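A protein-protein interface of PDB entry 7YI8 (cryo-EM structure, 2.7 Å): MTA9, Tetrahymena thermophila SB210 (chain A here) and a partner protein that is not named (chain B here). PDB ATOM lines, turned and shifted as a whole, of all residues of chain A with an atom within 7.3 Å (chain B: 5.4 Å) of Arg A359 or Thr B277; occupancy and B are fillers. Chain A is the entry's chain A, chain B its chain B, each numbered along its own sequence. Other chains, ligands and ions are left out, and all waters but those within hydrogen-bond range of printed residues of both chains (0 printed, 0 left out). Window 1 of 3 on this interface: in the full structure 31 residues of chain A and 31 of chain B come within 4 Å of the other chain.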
ATOM      1  N   SER A 188      32.342   4.134 -21.425  1.00  0.00           N
ATOM      2  CA  SER A 188      31.814   5.231 -20.632  1.00  0.00           C
ATOM      3  C   SER A 188      30.670   4.769 -19.741  1.00  0.00           C
ATOM      4  O   SER A 188      30.129   3.671 -19.891  1.00  0.00           O
ATOM      5  CB  SER A 188      31.330   6.365 -21.537  1.00  0.00           C
ATOM      6  OG  SER A 188      30.796   7.433 -20.778  1.00  0.00           O
ATOM      7  N   GLU A 189      30.313   5.632 -18.796  1.00  0.00           N
ATOM      8  CA  GLU A 189      29.120   5.472 -17.984  1.00  0.00           C
ATOM      9  C   GLU A 189      28.461   6.834 -17.841  1.00  0.00           C
ATOM     10  O   GLU A 189      29.105   7.873 -17.989  1.00  0.00           O
ATOM     11  CB  GLU A 189      29.436   4.876 -16.608  1.00  0.00           C
ATOM     12  CG  GLU A 189      29.953   3.447 -16.649  1.00  0.00           C
ATOM     13  CD  GLU A 189      28.874   2.445 -17.011  1.00  0.00           C
ATOM     14  OE1 GLU A 189      27.894   2.321 -16.247  1.00  0.00           O
ATOM     15  OE2 GLU A 189      29.009   1.777 -18.058  1.00  0.00           O
ATOM     16  N   LYS A 190      27.157   6.820 -17.559  1.00  0.00           N
ATOM     17  CA  LYS A 190      26.420   8.076 -17.459  1.00  0.00           C
ATOM     18  C   LYS A 190      26.903   8.926 -16.291  1.00  0.00           C
ATOM     19  O   LYS A 190      26.789  10.155 -16.334  1.00  0.00           O
ATOM     20  CB  LYS A 190      24.923   7.796 -17.332  1.00  0.00           C
ATOM     21  CG  LYS A 190      24.246   7.439 -18.647  1.00  0.00           C
ATOM     22  CD  LYS A 190      22.802   7.907 -18.669  1.00  0.00           C
ATOM     23  CE  LYS A 190      21.836   6.736 -18.602  1.00  0.00           C
ATOM     24  NZ  LYS A 190      20.419   7.188 -18.600  1.00  0.00           N
ATOM     25  N   LEU A 193      30.804  10.639 -17.462  1.00  0.00           N
ATOM     26  CA  LEU A 193      31.114  11.080 -18.819  1.00  0.00           C
ATOM     27  C   LEU A 193      31.894  12.392 -18.810  1.00  0.00           C
ATOM     28  O   LEU A 193      32.921  12.527 -19.493  1.00  0.00           O
ATOM     29  CB  LEU A 193      29.824  11.221 -19.628  1.00  0.00           C
ATOM     30  CG  LEU A 193      29.878  12.056 -20.910  1.00  0.00           C
ATOM     31  CD1 LEU A 193      30.673  11.350 -21.992  1.00  0.00           C
ATOM     32  CD2 LEU A 193      28.474  12.370 -21.397  1.00  0.00           C
ATOM     33  N   ASN A 210      31.394   9.026 -30.659  1.00  0.00           N
ATOM     34  CA  ASN A 210      30.683   8.173 -29.725  1.00  0.00           C
ATOM     35  C   ASN A 210      30.243   6.916 -30.463  1.00  0.00           C
ATOM     36  O   ASN A 210      30.171   6.890 -31.692  1.00  0.00           O
ATOM     37  CB  ASN A 210      29.476   8.907 -29.123  1.00  0.00           C
ATOM     38  CG  ASN A 210      28.899   8.194 -27.927  1.00  0.00           C
ATOM     39  OD1 ASN A 210      29.193   7.027 -27.684  1.00  0.00           O
ATOM     40  ND2 ASN A 210      28.069   8.896 -27.167  1.00  0.00           N
ATOM     41  N   PHE A 211      29.989   5.852 -29.704  1.00  0.00           N
ATOM     42  CA  PHE A 211      29.438   4.624 -30.263  1.00  0.00           C
ATOM     43  C   PHE A 211      28.465   4.038 -29.254  1.00  0.00           C
ATOM     44  O   PHE A 211      28.772   3.976 -28.061  1.00  0.00           O
ATOM     45  CB  PHE A 211      30.546   3.620 -30.600  1.00  0.00           C
ATOM     46  CG  PHE A 211      30.041   2.281 -31.047  1.00  0.00           C
ATOM     47  CD1 PHE A 211      29.580   2.096 -32.339  1.00  0.00           C
ATOM     48  CD2 PHE A 211      30.037   1.201 -30.180  1.00  0.00           C
ATOM     49  CE1 PHE A 211      29.117   0.864 -32.754  1.00  0.00           C
ATOM     50  CE2 PHE A 211      29.576  -0.032 -30.590  1.00  0.00           C
ATOM     51  CZ  PHE A 211      29.116  -0.201 -31.878  1.00  0.00           C
ATOM     52  N   SER A 212      27.294   3.617 -29.722  1.00  0.00           N
ATOM     53  CA  SER A 212      26.226   3.213 -28.821  1.00  0.00           C
ATOM     54  C   SER A 212      25.660   1.854 -29.203  1.00  0.00           C
ATOM     55  O   SER A 212      25.506   1.532 -30.390  1.00  0.00           O
ATOM     56  CB  SER A 212      25.104   4.254 -28.798  1.00  0.00           C
ATOM     57  OG  SER A 212      25.426   5.325 -27.927  1.00  0.00           O
ATOM     58  N   ILE A 213      25.354   1.066 -28.177  1.00  0.00           N
ATOM     59  CA  ILE A 213      24.692  -0.223 -28.323  1.00  0.00           C
ATOM     60  C   ILE A 213      23.319  -0.112 -27.678  1.00  0.00           C
ATOM     61  O   ILE A 213      23.217   0.163 -26.477  1.00  0.00           O
ATOM     62  CB  ILE A 213      25.506  -1.358 -27.683  1.00  0.00           C
ATOM     63  CG1 ILE A 213      26.970  -1.282 -28.113  1.00  0.00           C
ATOM     64  CG2 ILE A 213      24.912  -2.707 -28.046  1.00  0.00           C
ATOM     65  CD1 ILE A 213      27.883  -2.168 -27.299  1.00  0.00           C
ATOM     66  N   MET A 214      22.271  -0.327 -28.473  1.00  0.00           N
ATOM     67  CA  MET A 214      20.894  -0.348 -27.998  1.00  0.00           C
ATOM     68  C   MET A 214      20.537  -1.753 -27.538  1.00  0.00           C
ATOM     69  O   MET A 214      20.645  -2.714 -28.308  1.00  0.00           O
ATOM     70  CB  MET A 214      19.929   0.098 -29.097  1.00  0.00           C
ATOM     71  CG  MET A 214      20.044   1.553 -29.517  1.00  0.00           C
ATOM     72  SD  MET A 214      20.259   2.672 -28.124  1.00  0.00           S
ATOM     73  CE  MET A 214      21.591   3.702 -28.716  1.00  0.00           C
ATOM     74  N   PHE A 215      20.077  -1.860 -26.298  1.00  0.00           N
ATOM     75  CA  PHE A 215      19.891  -3.143 -25.638  1.00  0.00           C
ATOM     76  C   PHE A 215      18.426  -3.556 -25.656  1.00  0.00           C
ATOM     77  O   PHE A 215      17.553  -2.802 -25.214  1.00  0.00           O
ATOM     78  CB  PHE A 215      20.403  -3.080 -24.200  1.00  0.00           C
ATOM     79  CG  PHE A 215      21.894  -3.189 -24.086  1.00  0.00           C
ATOM     80  CD1 PHE A 215      22.616  -3.939 -24.996  1.00  0.00           C
ATOM     81  CD2 PHE A 215      22.574  -2.539 -23.072  1.00  0.00           C
ATOM     82  CE1 PHE A 215      23.987  -4.042 -24.896  1.00  0.00           C
ATOM     83  CE2 PHE A 215      23.944  -2.638 -22.968  1.00  0.00           C
ATOM     84  CZ  PHE A 215      24.651  -3.390 -23.881  1.00  0.00           C
ATOM     85  N   LEU A 348      15.323  -2.811 -22.978  1.00  0.00           N
ATOM     86  CA  LEU A 348      15.587  -2.919 -21.550  1.00  0.00           C
ATOM     87  C   LEU A 348      15.275  -1.614 -20.830  1.00  0.00           C
ATOM     88  O   LEU A 348      15.366  -0.523 -21.399  1.00  0.00           O
ATOM     89  CB  LEU A 348      17.041  -3.304 -21.274  1.00  0.00           C
ATOM     90  CG  LEU A 348      17.559  -4.674 -21.692  1.00  0.00           C
ATOM     91  CD1 LEU A 348      19.045  -4.752 -21.438  1.00  0.00           C
ATOM     92  CD2 LEU A 348      16.844  -5.731 -20.880  1.00  0.00           C
ATOM     93  N   ASN A 350      16.643  -0.446 -17.342  1.00  0.00           N
ATOM     94  CA  ASN A 350      17.470  -0.630 -16.159  1.00  0.00           C
ATOM     95  C   ASN A 350      17.343   0.566 -15.225  1.00  0.00           C
ATOM     96  O   ASN A 350      17.056   1.686 -15.651  1.00  0.00           O
ATOM     97  CB  ASN A 350      18.936  -0.835 -16.541  1.00  0.00           C
ATOM     98  CG  ASN A 350      19.163  -2.109 -17.329  1.00  0.00           C
ATOM     99  OD1 ASN A 350      19.540  -2.070 -18.499  1.00  0.00           O
ATOM    100  ND2 ASN A 350      18.936  -3.249 -16.688  1.00  0.00           N
ATOM    101  N   LYS A 356      15.932   5.573 -17.478  1.00  0.00           N
ATOM    102  CA  LYS A 356      16.088   4.124 -17.541  1.00  0.00           C
ATOM    103  C   LYS A 356      17.139   3.789 -18.591  1.00  0.00           C
ATOM    104  O   LYS A 356      17.038   4.235 -19.739  1.00  0.00           O
ATOM    105  CB  LYS A 356      14.757   3.442 -17.849  1.00  0.00           C
ATOM    106  CG  LYS A 356      13.970   3.102 -16.596  1.00  0.00           C
ATOM    107  CD  LYS A 356      12.551   2.686 -16.912  1.00  0.00           C
ATOM    108  CE  LYS A 356      11.852   2.170 -15.670  1.00  0.00           C
ATOM    109  NZ  LYS A 356      12.620   1.072 -15.026  1.00  0.00           N
ATOM    110  N   LYS A 357      18.145   3.017 -18.190  1.00  0.00           N
ATOM    111  CA  LYS A 357      19.259   2.702 -19.075  1.00  0.00           C
ATOM    112  C   LYS A 357      18.818   1.767 -20.194  1.00  0.00           C
ATOM    113  O   LYS A 357      18.166   0.748 -19.950  1.00  0.00           O
ATOM    114  CB  LYS A 357      20.397   2.066 -18.282  1.00  0.00           C
ATOM    115  CG  LYS A 357      21.468   3.041 -17.834  1.00  0.00           C
ATOM    116  CD  LYS A 357      22.607   2.319 -17.138  1.00  0.00           C
ATOM    117  CE  LYS A 357      22.129   1.651 -15.859  1.00  0.00           C
ATOM    118  NZ  LYS A 357      21.310   2.572 -15.026  1.00  0.00           N
ATOM    119  N   THR A 358      19.189   2.114 -21.424  1.00  0.00           N
ATOM    120  CA  THR A 358      18.899   1.280 -22.585  1.00  0.00           C
ATOM    121  C   THR A 358      20.078   1.122 -23.532  1.00  0.00           C
ATOM    122  O   THR A 358      20.038   0.237 -24.395  1.00  0.00           O
ATOM    123  CB  THR A 358      17.700   1.849 -23.360  1.00  0.00           C
ATOM    124  OG1 THR A 358      16.683   2.249 -22.434  1.00  0.00           O
ATOM    125  CG2 THR A 358      17.104   0.813 -24.300  1.00  0.00           C
ATOM    126  N   ARG A 359      21.136   1.917 -23.403  1.00  0.00           N
ATOM    127  CA  ARG A 359      22.281   1.838 -24.295  1.00  0.00           C
ATOM    128  C   ARG A 359      23.565   1.711 -23.489  1.00  0.00           C
ATOM    129  O   ARG A 359      23.610   1.993 -22.288  1.00  0.00           O
ATOM    130  CB  ARG A 359      22.384   3.065 -25.203  1.00  0.00           C
ATOM    131  CG  ARG A 359      22.294   4.368 -24.448  1.00  0.00           C
ATOM    132  CD  ARG A 359      22.852   5.528 -25.249  1.00  0.00           C
ATOM    133  NE  ARG A 359      23.181   6.643 -24.371  1.00  0.00           N
ATOM    134  CZ  ARG A 359      22.287   7.389 -23.737  1.00  0.00           C
ATOM    135  NH1 ARG A 359      20.991   7.243 -23.947  1.00  0.00           N
ATOM    136  NH2 ARG A 359      22.706   8.309 -22.874  1.00  0.00           N
ATOM    137  N   HIS A 360      24.610   1.273 -24.179  1.00  0.00           N
ATOM    138  CA  HIS A 360      25.968   1.268 -23.656  1.00  0.00           C
ATOM    139  C   HIS A 360      26.846   2.124 -24.555  1.00  0.00           C
ATOM    140  O   HIS A 360      26.701   2.100 -25.782  1.00  0.00           O
ATOM    141  CB  HIS A 360      26.538  -0.147 -23.557  1.00  0.00           C
ATOM    142  CG  HIS A 360      27.669  -0.267 -22.584  1.00  0.00           C
ATOM    143  ND1 HIS A 360      28.954  -0.584 -22.968  1.00  0.00           N
ATOM    144  CD2 HIS A 360      27.710  -0.098 -21.242  1.00  0.00           C
ATOM    145  CE1 HIS A 360      29.735  -0.613 -21.904  1.00  0.00           C
ATOM    146  NE2 HIS A 360      29.005  -0.321 -20.844  1.00  0.00           N
ATOM    147  N   THR A 361      27.760   2.869 -23.937  1.00  0.00           N
ATOM    148  CA  THR A 361      28.490   3.944 -24.591  1.00  0.00           C
ATOM    149  C   THR A 361      29.980   3.634 -24.650  1.00  0.00           C
ATOM    150  O   THR A 361      30.574   3.191 -23.664  1.00  0.00           O
ATOM    151  CB  THR A 361      28.270   5.272 -23.856  1.00  0.00           C
ATOM    152  OG1 THR A 361      26.865   5.524 -23.726  1.00  0.00           O
ATOM    153  CG2 THR A 361      28.913   6.419 -24.611  1.00  0.00           C
ATOM    154  N   ASP A 384      26.934   4.198 -36.481  1.00  0.00           N
ATOM    155  CA  ASP A 384      27.214   4.793 -35.182  1.00  0.00           C
ATOM    156  C   ASP A 384      26.433   4.124 -34.059  1.00  0.00           C
ATOM    157  O   ASP A 384      26.811   4.254 -32.891  1.00  0.00           O
ATOM    158  CB  ASP A 384      26.909   6.290 -35.240  1.00  0.00           C
ATOM    159  CG  ASP A 384      27.006   6.964 -33.897  1.00  0.00           C
ATOM    160  OD1 ASP A 384      26.010   7.579 -33.468  1.00  0.00           O
ATOM    161  OD2 ASP A 384      28.076   6.878 -33.270  1.00  0.00           O
ATOM    162  N   VAL A 385      25.366   3.400 -34.385  1.00  0.00           N
ATOM    163  CA  VAL A 385      24.543   2.714 -33.398  1.00  0.00           C
ATOM    164  C   VAL A 385      24.360   1.270 -33.839  1.00  0.00           C
ATOM    165  O   VAL A 385      24.207   0.990 -35.033  1.00  0.00           O
ATOM    166  CB  VAL A 385      23.182   3.419 -33.206  1.00  0.00           C
ATOM    167  CG1 VAL A 385      22.422   3.499 -34.523  1.00  0.00           C
ATOM    168  CG2 VAL A 385      22.352   2.714 -32.146  1.00  0.00           C
ATOM    169  N   VAL A 386      24.400   0.346 -32.878  1.00  0.00           N
ATOM    170  CA  VAL A 386      24.179  -1.066 -33.157  1.00  0.00           C
ATOM    171  C   VAL A 386      23.077  -1.555 -32.226  1.00  0.00           C
ATOM    172  O   VAL A 386      22.806  -0.957 -31.187  1.00  0.00           O
ATOM    173  CB  VAL A 386      25.464  -1.910 -32.984  1.00  0.00           C
ATOM    174  CG1 VAL A 386      25.865  -1.988 -31.520  1.00  0.00           C
ATOM    175  CG2 VAL A 386      25.308  -3.297 -33.594  1.00  0.00           C
ATOM    176  N   PRO A 395      24.566  -5.882 -18.462  1.00  0.00           N
ATOM    177  CA  PRO A 395      24.690  -5.416 -19.851  1.00  0.00           C
ATOM    178  C   PRO A 395      25.986  -4.675 -20.118  1.00  0.00           C
ATOM    179  O   PRO A 395      26.400  -4.579 -21.280  1.00  0.00           O
ATOM    180  CB  PRO A 395      23.470  -4.503 -20.025  1.00  0.00           C
ATOM    181  CG  PRO A 395      23.128  -4.062 -18.651  1.00  0.00           C
ATOM    182  CD  PRO A 395      23.495  -5.184 -17.733  1.00  0.00           C
ATOM    183  N   SER A 396      26.636  -4.143 -19.079  1.00  0.00           N
ATOM    184  CA  SER A 396      27.920  -3.475 -19.264  1.00  0.00           C
ATOM    185  C   SER A 396      28.998  -4.460 -19.693  1.00  0.00           C
ATOM    186  O   SER A 396      29.832  -4.142 -20.550  1.00  0.00           O
ATOM    187  CB  SER A 396      28.326  -2.761 -17.978  1.00  0.00           C
ATOM    188  OG  SER A 396      27.265  -1.964 -17.488  1.00  0.00           O
ATOM    189  N   ASP B 274      23.095  13.260 -17.459  1.00  0.00           N
ATOM    190  CA  ASP B 274      22.473  12.308 -18.369  1.00  0.00           C
ATOM    191  C   ASP B 274      22.573  12.842 -19.789  1.00  0.00           C
ATOM    192  O   ASP B 274      23.018  13.966 -20.021  1.00  0.00           O
ATOM    193  CB  ASP B 274      21.015  12.049 -17.972  1.00  0.00           C
ATOM    194  CG  ASP B 274      20.455  10.777 -18.577  1.00  0.00           C
ATOM    195  OD1 ASP B 274      20.916  10.374 -19.666  1.00  0.00           O
ATOM    196  OD2 ASP B 274      19.556  10.174 -17.957  1.00  0.00           O
ATOM    197  N   GLU B 275      22.163  12.012 -20.743  1.00  0.00           N
ATOM    198  CA  GLU B 275      21.917  12.499 -22.090  1.00  0.00           C
ATOM    199  C   GLU B 275      21.022  11.499 -22.805  1.00  0.00           C
ATOM    200  O   GLU B 275      21.168  10.286 -22.640  1.00  0.00           O
ATOM    201  CB  GLU B 275      23.225  12.754 -22.859  1.00  0.00           C
ATOM    202  CG  GLU B 275      24.134  11.567 -23.092  1.00  0.00           C
ATOM    203  CD  GLU B 275      23.766  10.795 -24.337  1.00  0.00           C
ATOM    204  OE1 GLU B 275      23.071  11.367 -25.200  1.00  0.00           O
ATOM    205  OE2 GLU B 275      24.184   9.625 -24.463  1.00  0.00           O
ATOM    206  N   ILE B 276      20.080  12.030 -23.577  1.00  0.00           N
ATOM    207  CA  ILE B 276      19.079  11.240 -24.284  1.00  0.00           C
ATOM    208  C   ILE B 276      19.506  11.120 -25.737  1.00  0.00           C
ATOM    209  O   ILE B 276      19.837  12.123 -26.379  1.00  0.00           O
ATOM    210  CB  ILE B 276      17.679  11.869 -24.180  1.00  0.00           C
ATOM    211  CG1 ILE B 276      17.090  11.660 -22.789  1.00  0.00           C
ATOM    212  CG2 ILE B 276      16.744  11.279 -25.217  1.00  0.00           C
ATOM    213  CD1 ILE B 276      15.894  12.536 -22.521  1.00  0.00           C
ATOM    214  N   THR B 277      19.499   9.897 -26.250  1.00  0.00           N
ATOM    215  CA  THR B 277      19.814   9.631 -27.644  1.00  0.00           C
ATOM    216  C   THR B 277      18.521   9.465 -28.429  1.00  0.00           C
ATOM    217  O   THR B 277      17.630   8.719 -28.012  1.00  0.00           O
ATOM    218  CB  THR B 277      20.677   8.376 -27.776  1.00  0.00           C
ATOM    219  OG1 THR B 277      21.901   8.559 -27.057  1.00  0.00           O
ATOM    220  CG2 THR B 277      20.986   8.099 -29.228  1.00  0.00           C
ATOM    221  N   TRP B 278      18.417  10.166 -29.553  1.00  0.00           N
ATOM    222  CA  TRP B 278      17.303  10.023 -30.478  1.00  0.00           C
ATOM    223  C   TRP B 278      17.823   9.328 -31.726  1.00  0.00           C
ATOM    224  O   TRP B 278      18.748   9.826 -32.377  1.00  0.00           O
ATOM    225  CB  TRP B 278      16.689  11.384 -30.814  1.00  0.00           C
ATOM    226  CG  TRP B 278      15.764  11.382 -32.002  1.00  0.00           C
ATOM    227  CD1 TRP B 278      14.898  10.394 -32.369  1.00  0.00           C
ATOM    228  CD2 TRP B 278      15.612  12.425 -32.973  1.00  0.00           C
ATOM    229  NE1 TRP B 278      14.224  10.752 -33.509  1.00  0.00           N
ATOM    230  CE2 TRP B 278      14.642  11.995 -33.899  1.00  0.00           C
ATOM    231  CE3 TRP B 278      16.202  13.679 -33.148  1.00  0.00           C
ATOM    232  CZ2 TRP B 278      14.249  12.775 -34.984  1.00  0.00           C
ATOM    233  CZ3 TRP B 278      15.811  14.451 -34.226  1.00  0.00           C
ATOM    234  CH2 TRP B 278      14.844  13.997 -35.129  1.00  0.00           C
ATOM    235  N   VAL B 279      17.234   8.177 -32.044  1.00  0.00           N
ATOM    236  CA  VAL B 279      17.601   7.364 -33.195  1.00  0.00           C
ATOM    237  C   VAL B 279      16.560   7.576 -34.285  1.00  0.00           C
ATOM    238  O   VAL B 279      15.345   7.582 -34.024  1.00  0.00           O
ATOM    239  CB  VAL B 279      17.715   5.876 -32.811  1.00  0.00           C
ATOM    240  CG1 VAL B 279      18.064   5.032 -34.025  1.00  0.00           C
ATOM    241  CG2 VAL B 279      18.742   5.687 -31.707  1.00  0.00           C
ATOM    242  N   LYS B 299      22.127   9.089 -35.077  1.00  0.00           N
ATOM    243  CA  LYS B 299      21.478   9.465 -33.830  1.00  0.00           C
ATOM    244  C   LYS B 299      21.895  10.881 -33.468  1.00  0.00           C
ATOM    245  O   LYS B 299      22.841  11.434 -34.034  1.00  0.00           O
ATOM    246  CB  LYS B 299      21.828   8.490 -32.702  1.00  0.00           C
ATOM    247  CG  LYS B 299      23.238   8.645 -32.164  1.00  0.00           C
ATOM    248  CD  LYS B 299      23.674   7.403 -31.408  1.00  0.00           C
ATOM    249  CE  LYS B 299      24.814   7.708 -30.456  1.00  0.00           C
ATOM    250  NZ  LYS B 299      26.016   8.192 -31.187  1.00  0.00           N
ATOM    251  N   GLU B 300      21.166  11.464 -32.519  1.00  0.00           N
ATOM    252  CA  GLU B 300      21.466  12.812 -32.054  1.00  0.00           C
ATOM    253  C   GLU B 300      21.234  12.898 -30.553  1.00  0.00           C
ATOM    254  O   GLU B 300      20.283  12.316 -30.030  1.00  0.00           O
ATOM    255  CB  GLU B 300      20.628  13.857 -32.799  1.00  0.00           C
ATOM    256  CG  GLU B 300      20.953  15.288 -32.420  1.00  0.00           C
ATOM    257  CD  GLU B 300      20.151  16.297 -33.210  1.00  0.00           C
ATOM    258  OE1 GLU B 300      19.322  15.879 -34.045  1.00  0.00           O
ATOM    259  OE2 GLU B 300      20.354  17.510 -32.998  1.00  0.00           O
ATOM    260  N   SER B 301      22.104  13.633 -29.865  1.00  0.00           N
ATOM    261  CA  SER B 301      22.167  13.619 -28.411  1.00  0.00           C
ATOM    262  C   SER B 301      21.655  14.924 -27.816  1.00  0.00           C
ATOM    263  O   SER B 301      21.941  16.013 -28.325  1.00  0.00           O
ATOM    264  CB  SER B 301      23.600  13.366 -27.935  1.00  0.00           C
ATOM    265  OG  SER B 301      24.125  12.178 -28.503  1.00  0.00           O
ATOM    266  N   CYS B 302      20.895  14.798 -26.731  1.00  0.00           N
ATOM    267  CA  CYS B 302      20.435  15.926 -25.930  1.00  0.00           C
ATOM    268  C   CYS B 302      20.998  15.749 -24.525  1.00  0.00           C
ATOM    269  O   CYS B 302      20.541  14.880 -23.777  1.00  0.00           O
ATOM    270  CB  CYS B 302      18.909  16.000 -25.912  1.00  0.00           C
ATOM    271  SG  CYS B 302      18.213  17.100 -24.661  1.00  0.00           S
ATOM    272  N   ASP B 322      16.112   6.199 -22.013  1.00  0.00           N
ATOM    273  CA  ASP B 322      16.952   7.267 -22.530  1.00  0.00           C
ATOM    274  C   ASP B 322      17.178   7.158 -24.032  1.00  0.00           C
ATOM    275  O   ASP B 322      18.106   7.779 -24.559  1.00  0.00           O
ATOM    276  CB  ASP B 322      18.286   7.291 -21.776  1.00  0.00           C
ATOM    277  CG  ASP B 322      19.092   6.014 -21.959  1.00  0.00           C
ATOM    278  OD1 ASP B 322      18.615   5.082 -22.636  1.00  0.00           O
ATOM    279  OD2 ASP B 322      20.213   5.941 -21.416  1.00  0.00           O
ATOM    280  N   VAL B 323      16.355   6.375 -24.724  1.00  0.00           N
ATOM    281  CA  VAL B 323      16.436   6.202 -26.170  1.00  0.00           C
ATOM    282  C   VAL B 323      15.081   6.550 -26.767  1.00  0.00           C
ATOM    283  O   VAL B 323      14.041   6.112 -26.261  1.00  0.00           O
ATOM    284  CB  VAL B 323      16.855   4.770 -26.550  1.00  0.00           C
ATOM    285  CG1 VAL B 323      16.984   4.637 -28.058  1.00  0.00           C
ATOM    286  CG2 VAL B 323      18.162   4.412 -25.876  1.00  0.00           C
ATOM    287  N   ILE B 324      15.096   7.344 -27.830  1.00  0.00           N
ATOM    288  CA  ILE B 324      13.892   7.782 -28.524  1.00  0.00           C
ATOM    289  C   ILE B 324      14.015   7.287 -29.958  1.00  0.00           C
ATOM    290  O   ILE B 324      14.731   7.885 -30.765  1.00  0.00           O
ATOM    291  CB  ILE B 324      13.719   9.303 -28.470  1.00  0.00           C
ATOM    292  CG1 ILE B 324      13.416   9.753 -27.044  1.00  0.00           C
ATOM    293  CG2 ILE B 324      12.630   9.755 -29.412  1.00  0.00           C
ATOM    294  CD1 ILE B 324      13.406  11.248 -26.861  1.00  0.00           C
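The side-chain amino group (NZ) of Lys A190 is in salt-bridge range of the side-chain carboxylate (OD2) of Asp B274, at 3.2 Å. The side-chain carboxylate (OD2) of Asp B322 is in salt-bridge range of the guanidinium group (NH1) of Arg A359 (3.0 Å). The guanidinium group of Arg A359 is in hydrogen-bond range of the side-chain hydroxyl of Thr B277, at 3.5 Å. OD1 of Asp B322 is in hydrogen-bond range of N of Thr A358 (3.3 Å). OD2 of Asp A384 lies within salt-bridge range of NZ of Lys B299, at 3.2 Å. The side-chain carboxylate of Asp B322 lies within salt-bridge range of the side-chain amino group of Lys A190. N of Asp B322 sits at hydrogen-bond distance from O of Lys A356 (3.1 Å). The guanidinium group (NH2) of Arg A359 lies within salt-bridge range of the side-chain carboxylate (OE2) of Glu B275, at 2.5 Å.
O of Leu A348 sits at hydrogen-bond distance from OG1 of Thr A358 (3.2 Å). The backbone NH of Ile B324 is in hydrogen-bond range of the backbone carbonyl oxygen of Thr B277 (2.9 Å). The side-chain carboxylate (OD2) of Asp A384 lies close to the backbone carbonyl oxygen (O) of Asn A210 (2.6 Å). OG1 of Thr A358 sits at hydrogen-bond distance from O of Lys A356, 3.4 Å away. N of Met A214 is in hydrogen-bond range of O of Val A386 (2.8 Å). The backbone NH (N) of Phe A215 is in hydrogen-bond range of the backbone carbonyl oxygen (O) of Thr A358, at 2.8 Å.
Ser A212 touches Lys B299 (OG to CE, 3.5 Å). Met A214 touches Val B323 (SD to CG2, 3.5 Å). Thr A358 touches Val B323 (CB to CG2, 3.6 Å).
Arg A359 touches just these residues of chain B: Glu B275 (2.5 Å), Thr B277 (3.5 Å) and Asp B322 (3.0 Å). Of the printed residues of chain B, Lys A356 touches Asp B322 (3.1 Å). Of the printed residues of chain A, Asp B274 touches Lys A190. Lys A357 touches none of the printed residues of chain B.
Of the 13 printed residues of chain B, 6 touch a printed residue of chain A. Hydrophobic or aromatic side chains of chain B that line the printed part of chain A: Val B323. Printed residues of chain A that touch a printed residue of chain B: Lys A190, Ser A212, Met A214, Lys A356, Thr A358, Arg A359 and Asp A384. Hydrophobic or aromatic side chains of chain A that line the printed part of chain B: Met A214. Among the printed residues, 11 pairs touch across the chains.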
